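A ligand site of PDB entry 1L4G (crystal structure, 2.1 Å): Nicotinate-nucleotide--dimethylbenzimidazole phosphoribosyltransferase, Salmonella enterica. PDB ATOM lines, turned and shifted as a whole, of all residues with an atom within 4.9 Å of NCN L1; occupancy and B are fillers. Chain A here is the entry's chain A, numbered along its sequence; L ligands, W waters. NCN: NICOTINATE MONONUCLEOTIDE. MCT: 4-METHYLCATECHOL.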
ATOM      1  N   VAL A  77      23.881 -36.344 -30.036  1.00  0.00           N
ATOM      2  CA  VAL A  77      24.067 -34.897 -30.233  1.00  0.00           C
ATOM      3  C   VAL A  77      23.652 -34.029 -29.042  1.00  0.00           C
ATOM      4  O   VAL A  77      23.789 -32.813 -29.089  1.00  0.00           O
ATOM      5  CB  VAL A  77      23.325 -34.393 -31.502  1.00  0.00           C
ATOM      6  CG1 VAL A  77      23.908 -35.033 -32.744  1.00  0.00           C
ATOM      7  CG2 VAL A  77      21.833 -34.697 -31.403  1.00  0.00           C
ATOM      8  N   ALA A  78      23.148 -34.659 -27.975  1.00  0.00           N
ATOM      9  CA  ALA A  78      22.716 -33.924 -26.777  1.00  0.00           C
ATOM     10  C   ALA A  78      23.088 -34.670 -25.497  1.00  0.00           C
ATOM     11  O   ALA A  78      22.843 -35.871 -25.378  1.00  0.00           O
ATOM     12  CB  ALA A  78      21.213 -33.683 -26.817  1.00  0.00           C
ATOM     13  N   GLU A 174      10.202 -22.841 -26.872  1.00  0.00           N
ATOM     14  CA  GLU A 174      10.230 -24.289 -26.998  1.00  0.00           C
ATOM     15  C   GLU A 174      10.948 -25.014 -25.866  1.00  0.00           C
ATOM     16  O   GLU A 174      11.540 -24.399 -24.988  1.00  0.00           O
ATOM     17  CB  GLU A 174      10.890 -24.684 -28.325  1.00  0.00           C
ATOM     18  CG  GLU A 174      12.150 -23.902 -28.669  1.00  0.00           C
ATOM     19  CD  GLU A 174      13.205 -24.006 -27.574  1.00  0.00           C
ATOM     20  OE1 GLU A 174      13.716 -25.103 -27.329  1.00  0.00           O
ATOM     21  OE2 GLU A 174      13.531 -22.981 -26.962  1.00  0.00           O
ATOM     22  N   LEU A 175      10.882 -26.339 -25.944  1.00  0.00           N
ATOM     23  CA  LEU A 175      11.502 -27.225 -24.982  1.00  0.00           C
ATOM     24  C   LEU A 175      11.634 -28.599 -25.637  1.00  0.00           C
ATOM     25  O   LEU A 175      10.634 -29.224 -26.001  1.00  0.00           O
ATOM     26  CB  LEU A 175      10.631 -27.320 -23.728  1.00  0.00           C
ATOM     27  CG  LEU A 175      11.169 -28.180 -22.584  1.00  0.00           C
ATOM     28  CD1 LEU A 175      12.487 -27.585 -22.081  1.00  0.00           C
ATOM     29  CD2 LEU A 175      10.134 -28.229 -21.457  1.00  0.00           C
ATOM     30  N   GLY A 176      12.863 -29.072 -25.802  1.00  0.00           N
ATOM     31  CA  GLY A 176      13.071 -30.374 -26.433  1.00  0.00           C
ATOM     32  C   GLY A 176      14.542 -30.713 -26.581  1.00  0.00           C
ATOM     33  O   GLY A 176      15.243 -30.125 -27.405  1.00  0.00           O
ATOM     34  N   MET A 177      15.009 -31.695 -25.798  1.00  0.00           N
ATOM     35  CA  MET A 177      16.402 -32.123 -25.845  1.00  0.00           C
ATOM     36  C   MET A 177      16.812 -32.495 -27.274  1.00  0.00           C
ATOM     37  O   MET A 177      16.110 -33.247 -27.960  1.00  0.00           O
ATOM     38  CB  MET A 177      16.627 -33.332 -24.911  1.00  0.00           C
ATOM     39  CG  MET A 177      16.102 -33.165 -23.494  1.00  0.00           C
ATOM     40  SD  MET A 177      16.758 -31.686 -22.659  1.00  0.00           S
ATOM     41  CE  MET A 177      15.384 -30.532 -22.888  1.00  0.00           C
ATOM     42  N   ALA A 178      17.954 -31.954 -27.712  1.00  0.00           N
ATOM     43  CA  ALA A 178      18.526 -32.181 -29.034  1.00  0.00           C
ATOM     44  C   ALA A 178      17.979 -31.309 -30.160  1.00  0.00           C
ATOM     45  O   ALA A 178      18.344 -31.523 -31.325  1.00  0.00           O
ATOM     46  CB  ALA A 178      18.396 -33.661 -29.431  1.00  0.00           C
ATOM     47  N   ASN A 179      17.117 -30.340 -29.841  1.00  0.00           N
ATOM     48  CA  ASN A 179      16.535 -29.524 -30.925  1.00  0.00           C
ATOM     49  C   ASN A 179      17.447 -28.498 -31.622  1.00  0.00           C
ATOM     50  O   ASN A 179      17.074 -27.973 -32.662  1.00  0.00           O
ATOM     51  CB  ASN A 179      15.200 -28.865 -30.479  1.00  0.00           C
ATOM     52  CG  ASN A 179      15.354 -27.819 -29.397  1.00  0.00           C
ATOM     53  OD1 ASN A 179      16.461 -27.411 -29.043  1.00  0.00           O
ATOM     54  ND2 ASN A 179      14.225 -27.357 -28.889  1.00  0.00           N
ATOM     55  N   THR A 180      18.635 -28.232 -31.075  1.00  0.00           N
ATOM     56  CA  THR A 180      19.524 -27.286 -31.747  1.00  0.00           C
ATOM     57  C   THR A 180      20.146 -27.979 -32.968  1.00  0.00           C
ATOM     58  O   THR A 180      20.822 -27.353 -33.793  1.00  0.00           O
ATOM     59  CB  THR A 180      20.655 -26.754 -30.834  1.00  0.00           C
ATOM     60  OG1 THR A 180      21.457 -27.834 -30.346  1.00  0.00           O
ATOM     61  CG2 THR A 180      20.071 -25.982 -29.652  1.00  0.00           C
ATOM     62  N   THR A 181      19.939 -29.291 -33.078  1.00  0.00           N
ATOM     63  CA  THR A 181      20.453 -30.033 -34.237  1.00  0.00           C
ATOM     64  C   THR A 181      19.545 -29.786 -35.450  1.00  0.00           C
ATOM     65  O   THR A 181      20.005 -29.319 -36.494  1.00  0.00           O
ATOM     66  CB  THR A 181      20.570 -31.546 -33.918  1.00  0.00           C
ATOM     67  OG1 THR A 181      21.721 -31.759 -33.075  1.00  0.00           O
ATOM     68  CG2 THR A 181      20.754 -32.368 -35.205  1.00  0.00           C
ATOM     69  N   ILE A 201      26.930 -25.356 -29.428  1.00  0.00           N
ATOM     70  CA  ILE A 201      27.055 -26.245 -28.264  1.00  0.00           C
ATOM     71  C   ILE A 201      25.711 -26.626 -27.645  1.00  0.00           C
ATOM     72  O   ILE A 201      25.652 -27.490 -26.771  1.00  0.00           O
ATOM     73  CB  ILE A 201      27.947 -25.591 -27.195  1.00  0.00           C
ATOM     74  N   GLY A 202      24.633 -25.986 -28.085  1.00  0.00           N
ATOM     75  CA  GLY A 202      23.330 -26.285 -27.534  1.00  0.00           C
ATOM     76  C   GLY A 202      23.359 -26.189 -26.018  1.00  0.00           C
ATOM     77  O   GLY A 202      23.867 -25.213 -25.479  1.00  0.00           O
ATOM     78  N   ALA A 203      22.832 -27.198 -25.341  1.00  0.00           N
ATOM     79  CA  ALA A 203      22.806 -27.218 -23.883  1.00  0.00           C
ATOM     80  C   ALA A 203      24.073 -27.861 -23.321  1.00  0.00           C
ATOM     81  O   ALA A 203      24.082 -29.017 -22.895  1.00  0.00           O
ATOM     82  CB  ALA A 203      21.566 -27.971 -23.390  1.00  0.00           C
ATOM     83  N   LYS A 213      28.127 -33.903 -34.197  1.00  0.00           N
ATOM     84  CA  LYS A 213      26.904 -33.133 -34.416  1.00  0.00           C
ATOM     85  C   LYS A 213      26.884 -32.581 -35.849  1.00  0.00           C
ATOM     86  O   LYS A 213      25.860 -32.646 -36.543  1.00  0.00           O
ATOM     87  CB  LYS A 213      26.807 -32.006 -33.396  1.00  0.00           C
ATOM     88  CG  LYS A 213      25.465 -31.279 -33.359  1.00  0.00           C
ATOM     89  CD  LYS A 213      25.374 -30.417 -32.120  1.00  0.00           C
ATOM     90  CE  LYS A 213      24.202 -29.458 -32.164  1.00  0.00           C
ATOM     91  NZ  LYS A 213      24.156 -28.587 -30.950  1.00  0.00           N
ATOM     92  N   ASP A 263      12.432 -15.637 -29.650  1.00  0.00           N
ATOM     93  CA  ASP A 263      13.218 -15.927 -28.457  1.00  0.00           C
ATOM     94  C   ASP A 263      14.667 -16.120 -28.914  1.00  0.00           C
ATOM     95  O   ASP A 263      15.297 -15.160 -29.348  1.00  0.00           O
ATOM     96  CB  ASP A 263      12.666 -17.163 -27.728  1.00  0.00           C
ATOM     97  CG  ASP A 263      13.449 -17.500 -26.455  1.00  0.00           C
ATOM     98  OD1 ASP A 263      13.896 -16.561 -25.750  1.00  0.00           O
ATOM     99  OD2 ASP A 263      13.584 -18.694 -26.124  1.00  0.00           O
ATOM    100  N   GLY A 264      15.163 -17.353 -28.849  1.00  0.00           N
ATOM    101  CA  GLY A 264      16.530 -17.626 -29.258  1.00  0.00           C
ATOM    102  C   GLY A 264      16.755 -18.310 -30.587  1.00  0.00           C
ATOM    103  O   GLY A 264      15.949 -18.198 -31.520  1.00  0.00           O
ATOM    104  N   PHE A 265      17.859 -19.051 -30.660  1.00  0.00           N
ATOM    105  CA  PHE A 265      18.248 -19.773 -31.878  1.00  0.00           C
ATOM    106  C   PHE A 265      17.166 -20.645 -32.496  1.00  0.00           C
ATOM    107  O   PHE A 265      16.941 -20.609 -33.709  1.00  0.00           O
ATOM    108  CB  PHE A 265      19.503 -20.615 -31.615  1.00  0.00           C
ATOM    109  CG  PHE A 265      20.106 -21.224 -32.867  1.00  0.00           C
ATOM    110  CD1 PHE A 265      20.049 -22.595 -33.088  1.00  0.00           C
ATOM    111  CD2 PHE A 265      20.685 -20.418 -33.842  1.00  0.00           C
ATOM    112  CE1 PHE A 265      20.562 -23.147 -34.266  1.00  0.00           C
ATOM    113  CE2 PHE A 265      21.197 -20.961 -35.022  1.00  0.00           C
ATOM    114  CZ  PHE A 265      21.139 -22.329 -35.229  1.00  0.00           C
ATOM    115  N   LEU A 266      16.493 -21.454 -31.667  1.00  0.00           N
ATOM    116  CA  LEU A 266      15.429 -22.324 -32.167  1.00  0.00           C
ATOM    117  C   LEU A 266      14.316 -21.507 -32.794  1.00  0.00           C
ATOM    118  O   LEU A 266      13.744 -21.901 -33.810  1.00  0.00           O
ATOM    119  CB  LEU A 266      14.848 -23.182 -31.032  1.00  0.00           C
ATOM    120  CG  LEU A 266      15.665 -24.347 -30.455  1.00  0.00           C
ATOM    121  CD1 LEU A 266      16.067 -25.295 -31.575  1.00  0.00           C
ATOM    122  CD2 LEU A 266      16.879 -23.842 -29.723  1.00  0.00           C
ATOM    123  N   SER A 291      20.868 -14.730 -29.022  1.00  0.00           N
ATOM    124  CA  SER A 291      21.264 -16.026 -28.473  1.00  0.00           C
ATOM    125  C   SER A 291      22.768 -16.277 -28.604  1.00  0.00           C
ATOM    126  O   SER A 291      23.394 -15.876 -29.583  1.00  0.00           O
ATOM    127  CB  SER A 291      20.492 -17.137 -29.196  1.00  0.00           C
ATOM    128  OG  SER A 291      20.975 -18.428 -28.827  1.00  0.00           O
ATOM    129  N   GLU A 293      24.101 -19.000 -29.130  1.00  0.00           N
ATOM    130  CA  GLU A 293      24.330 -20.134 -30.019  1.00  0.00           C
ATOM    131  C   GLU A 293      25.172 -19.643 -31.215  1.00  0.00           C
ATOM    132  O   GLU A 293      24.932 -18.569 -31.759  1.00  0.00           O
ATOM    133  CB  GLU A 293      22.983 -20.675 -30.498  1.00  0.00           C
ATOM    134  CG  GLU A 293      23.047 -21.957 -31.292  1.00  0.00           C
ATOM    135  CD  GLU A 293      23.337 -23.174 -30.436  1.00  0.00           C
ATOM    136  OE1 GLU A 293      23.355 -24.290 -30.968  1.00  0.00           O
ATOM    137  OE2 GLU A 293      23.554 -23.056 -29.215  1.00  0.00           O
ATOM    138  N   MET A 313      22.287 -15.291 -23.451  1.00  0.00           N
ATOM    139  CA  MET A 313      21.393 -16.350 -22.998  1.00  0.00           C
ATOM    140  C   MET A 313      21.252 -17.464 -24.009  1.00  0.00           C
ATOM    141  O   MET A 313      21.359 -17.247 -25.212  1.00  0.00           O
ATOM    142  CB  MET A 313      20.012 -15.769 -22.681  1.00  0.00           C
ATOM    143  CG  MET A 313      20.017 -14.844 -21.471  1.00  0.00           C
ATOM    144  SD  MET A 313      18.503 -13.866 -21.208  1.00  0.00           S
ATOM    145  CE  MET A 313      17.327 -15.216 -20.886  1.00  0.00           C
ATOM    146  N   ARG A 314      21.011 -18.678 -23.519  1.00  0.00           N
ATOM    147  CA  ARG A 314      20.864 -19.856 -24.375  1.00  0.00           C
ATOM    148  C   ARG A 314      20.061 -20.929 -23.651  1.00  0.00           C
ATOM    149  O   ARG A 314      20.354 -22.116 -23.745  1.00  0.00           O
ATOM    150  CB  ARG A 314      22.260 -20.386 -24.758  1.00  0.00           C
ATOM    151  CG  ARG A 314      23.201 -20.584 -23.571  1.00  0.00           C
ATOM    152  CD  ARG A 314      24.628 -20.928 -24.012  1.00  0.00           C
ATOM    153  NE  ARG A 314      25.585 -20.925 -22.902  1.00  0.00           N
ATOM    154  CZ  ARG A 314      25.672 -21.869 -21.971  1.00  0.00           C
ATOM    155  NH1 ARG A 314      24.861 -22.916 -21.988  1.00  0.00           N
ATOM    156  NH2 ARG A 314      26.577 -21.775 -21.012  1.00  0.00           N
ATOM    157  N   LEU A 315      19.035 -20.489 -22.918  1.00  0.00           N
ATOM    158  CA  LEU A 315      18.180 -21.400 -22.178  1.00  0.00           C
ATOM    159  C   LEU A 315      16.998 -21.946 -22.978  1.00  0.00           C
ATOM    160  O   LEU A 315      16.693 -23.135 -22.932  1.00  0.00           O
ATOM    161  CB  LEU A 315      17.641 -20.706 -20.933  1.00  0.00           C
ATOM    162  CG  LEU A 315      16.548 -21.458 -20.166  1.00  0.00           C
ATOM    163  CD1 LEU A 315      17.102 -22.749 -19.551  1.00  0.00           C
ATOM    164  CD2 LEU A 315      16.002 -20.557 -19.074  1.00  0.00           C
ATOM    165  N   GLY A 316      16.321 -21.053 -23.709  1.00  0.00           N
ATOM    166  CA  GLY A 316      15.156 -21.448 -24.469  1.00  0.00           C
ATOM    167  C   GLY A 316      13.927 -21.173 -23.606  1.00  0.00           C
ATOM    168  O   GLY A 316      13.960 -20.281 -22.756  1.00  0.00           O
ATOM    169  N   GLU A 317      12.866 -21.960 -23.825  1.00  0.00           N
ATOM    170  CA  GLU A 317      11.586 -21.829 -23.108  1.00  0.00           C
ATOM    171  C   GLU A 317      10.838 -20.544 -23.454  1.00  0.00           C
ATOM    172  O   GLU A 317       9.691 -20.352 -23.023  1.00  0.00           O
ATOM    173  CB  GLU A 317      11.827 -21.859 -21.591  1.00  0.00           C
ATOM    174  CG  GLU A 317      12.745 -22.953 -21.117  1.00  0.00           C
ATOM    175  CD  GLU A 317      12.806 -23.040 -19.609  1.00  0.00           C
ATOM    176  OE1 GLU A 317      12.372 -22.085 -18.941  1.00  0.00           O
ATOM    177  OE2 GLU A 317      13.285 -24.057 -19.078  1.00  0.00           O
HETATM  178  P   NCN L   1      20.500 -29.399 -27.170  1.00  0.00           P
HETATM  179  O1P NCN L   1      20.410 -29.484 -28.651  1.00  0.00           O
HETATM  180  O2P NCN L   1      21.932 -29.465 -26.757  1.00  0.00           O
HETATM  181  O3P NCN L   1      19.680 -30.632 -26.471  1.00  0.00           O
HETATM  182  O5' NCN L   1      19.905 -28.020 -26.672  1.00  0.00           O
HETATM  183  C5' NCN L   1      18.529 -27.692 -26.960  1.00  0.00           C
HETATM  184  C4' NCN L   1      17.833 -27.494 -25.739  1.00  0.00           C
HETATM  185  O4' NCN L   1      18.492 -26.469 -24.940  1.00  0.00           O
HETATM  186  C3' NCN L   1      16.384 -27.086 -25.839  1.00  0.00           C
HETATM  187  O3' NCN L   1      15.553 -27.688 -24.810  1.00  0.00           O
HETATM  188  C2' NCN L   1      16.477 -25.533 -25.747  1.00  0.00           C
HETATM  189  O2' NCN L   1      15.350 -25.034 -24.984  1.00  0.00           O
HETATM  190  C1' NCN L   1      17.855 -25.236 -25.114  1.00  0.00           C
HETATM  191  N1  NCN L   1      18.772 -24.291 -25.861  1.00  0.00           N
HETATM  192  C6  NCN L   1      20.162 -24.591 -26.097  1.00  0.00           C
HETATM  193  C5  NCN L   1      20.848 -23.594 -26.798  1.00  0.00           C
HETATM  194  C4  NCN L   1      20.309 -22.358 -27.279  1.00  0.00           C
HETATM  195  C3  NCN L   1      18.889 -22.188 -26.959  1.00  0.00           C
HETATM  196  C2  NCN L   1      18.141 -23.131 -26.274  1.00  0.00           C
HETATM  197  C7  NCN L   1      18.460 -20.836 -27.522  1.00  0.00           C
HETATM  198  O7  NCN L   1      19.126 -20.026 -28.120  1.00  0.00           O
HETATM  199  O8  NCN L   1      17.177 -20.662 -27.238  1.00  0.00           O
HETATM  200  C1  MCT L   2      16.634 -27.873 -18.481  1.00  0.00           C
HETATM  201  C2  MCT L   2      15.854 -26.758 -18.851  1.00  0.00           C
HETATM  202  C3  MCT L   2      15.867 -26.310 -20.140  1.00  0.00           C
HETATM  203  O3  MCT L   2      15.066 -25.162 -20.540  1.00  0.00           O
HETATM  204  C4  MCT L   2      16.664 -26.973 -21.103  1.00  0.00           C
HETATM  205  O4  MCT L   2      16.630 -26.453 -22.424  1.00  0.00           O
HETATM  206  C5  MCT L   2      17.439 -28.075 -20.772  1.00  0.00           C
HETATM  207  C6  MCT L   2      17.440 -28.539 -19.464  1.00  0.00           C
HETATM  208  C   MCT L   2      16.636 -28.387 -17.056  1.00  0.00           C
HETATM  209  O   HOH W   1      20.843 -31.607 -24.281  1.00  0.00           O
HETATM  210  O   HOH W   2      23.423 -31.022 -24.987  1.00  0.00           O
HETATM  211  O   HOH W   3      15.032 -20.264 -28.982  1.00  0.00           O
HETATM  212  O   HOH W   4      23.941 -30.123 -28.547  1.00  0.00           O
HETATM  213  O   HOH W   5      21.703 -31.376 -30.358  1.00  0.00           O
HETATM  214  O   HOH W   6      16.339 -18.425 -25.797  1.00  0.00           O
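An oxygen (O4) of MCT L2 lies within hydrogen-bond range of the backbone carbonyl oxygen (O) of Leu 315, 3.4 Å away. The backbone NH (N) of Ala 178 lies within hydrogen-bond range of an oxygen (O3P) of NCN L1 (2.5 Å). An oxygen (O7) of NCN L1 is in hydrogen-bond range of the backbone NH (N) of Phe 265 (3.0 Å). O1P of NCN L1 sits at hydrogen-bond distance from N of Thr 180. O3' of NCN L1 sits at hydrogen-bond distance from N of Gly 176. O2P of NCN L1 is in hydrogen-bond range of N of Ala 203, at 2.8 Å. An oxygen (O1P) of NCN L1 lies within hydrogen-bond range of the side-chain hydroxyl (OG1) of Thr 180, at 2.6 Å. OG of Ser 291 lies within hydrogen-bond range of O7 of NCN L1 (2.5 Å). OE1 of Glu 174 sits at hydrogen-bond distance from O2' of NCN L1 (2.9 Å). The backbone carbonyl oxygen of Leu 315 sits at hydrogen-bond distance from an oxygen (O2') of NCN L1 (3.1 Å). An oxygen (O3) of MCT L2 lies within hydrogen-bond range of the side-chain carboxylate (OE2) of Glu 317, 2.6 Å away.
O4 of MCT L2 lies within hydrogen-bond range of O3' of NCN L1 (2.9 Å).
Water W4 lies within hydrogen-bond range of the backbone carbonyl oxygen (O) of Val 77 (2.7 Å), an oxygen (O2P) of NCN L1 (2.8 Å) and the side-chain amino group (NZ) of Lys 213 (2.9 Å). Water W2 bridges O2P of NCN L1 (2.8 Å) and O of Ala 203 (3.0 Å). Water W6 lies within hydrogen-bond range of the side-chain carboxylate of Asp 263 (2.8 Å), an oxygen (O8) of NCN L1 (2.8 Å), the backbone NH of Gly 316 (3.4 Å) and the backbone NH of Gly 264 (3.4 Å). Water W3 lies within hydrogen-bond range of an oxygen (O8) of NCN L1 (2.8 Å), the backbone NH (N) of Gly 264 (2.9 Å) and the backbone NH (N) of Leu 266 (3.3 Å). Water W5 lies within hydrogen-bond range of the side-chain hydroxyl of Thr 181 (2.7 Å), the backbone carbonyl oxygen of Val 77 (2.8 Å), an oxygen (O1P) of NCN L1 (2.9 Å) and the backbone carbonyl oxygen of Ala 178 (3.5 Å).
The side-chain amino group (NZ) of Lys 213 sits at hydrogen-bond distance from the side-chain hydroxyl (OG1) of Thr 180, 2.9 Å away. The side-chain amide nitrogen (ND2) of Asn 179 lies within hydrogen-bond range of the side-chain carboxylate (OE1) of Glu 174, at 2.8 Å. ND2 of Asn 179 lies close to O of Gly 176, at 3.3 Å. N of Gly 202 lies within hydrogen-bond range of OE2 of Glu 293 (3.3 Å). The backbone NH (N) of Glu 317 lies within hydrogen-bond range of the backbone carbonyl oxygen (O) of Glu 174. The backbone NH (N) of Glu 293 sits close to the side-chain hydroxyl (OG) of Ser 291, at 3.2 Å.
The backbone carbonyl oxygen (O) of Arg 314 sits close to a nitrogen (N1) of NCN L1 (3.4 Å). CB of Ala 78 touches O3P of NCN L1, at 3.4 Å. Met 177 touches NCN L1. OD1 of Asn 179 touches C5' of NCN L1, at 2.9 Å. CA of Gly 202 touches O2P of NCN L1 (3.6 Å). Gly 264 touches NCN L1. Leu 266 touches NCN L1. OE2 of Glu 293 touches C5 of NCN L1, at 3.7 Å. Gly 316 touches NCN L1 (CA to O8, 3.5 Å). Of the 25 residues printed, 17 come within 4 Å of NCN L1.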
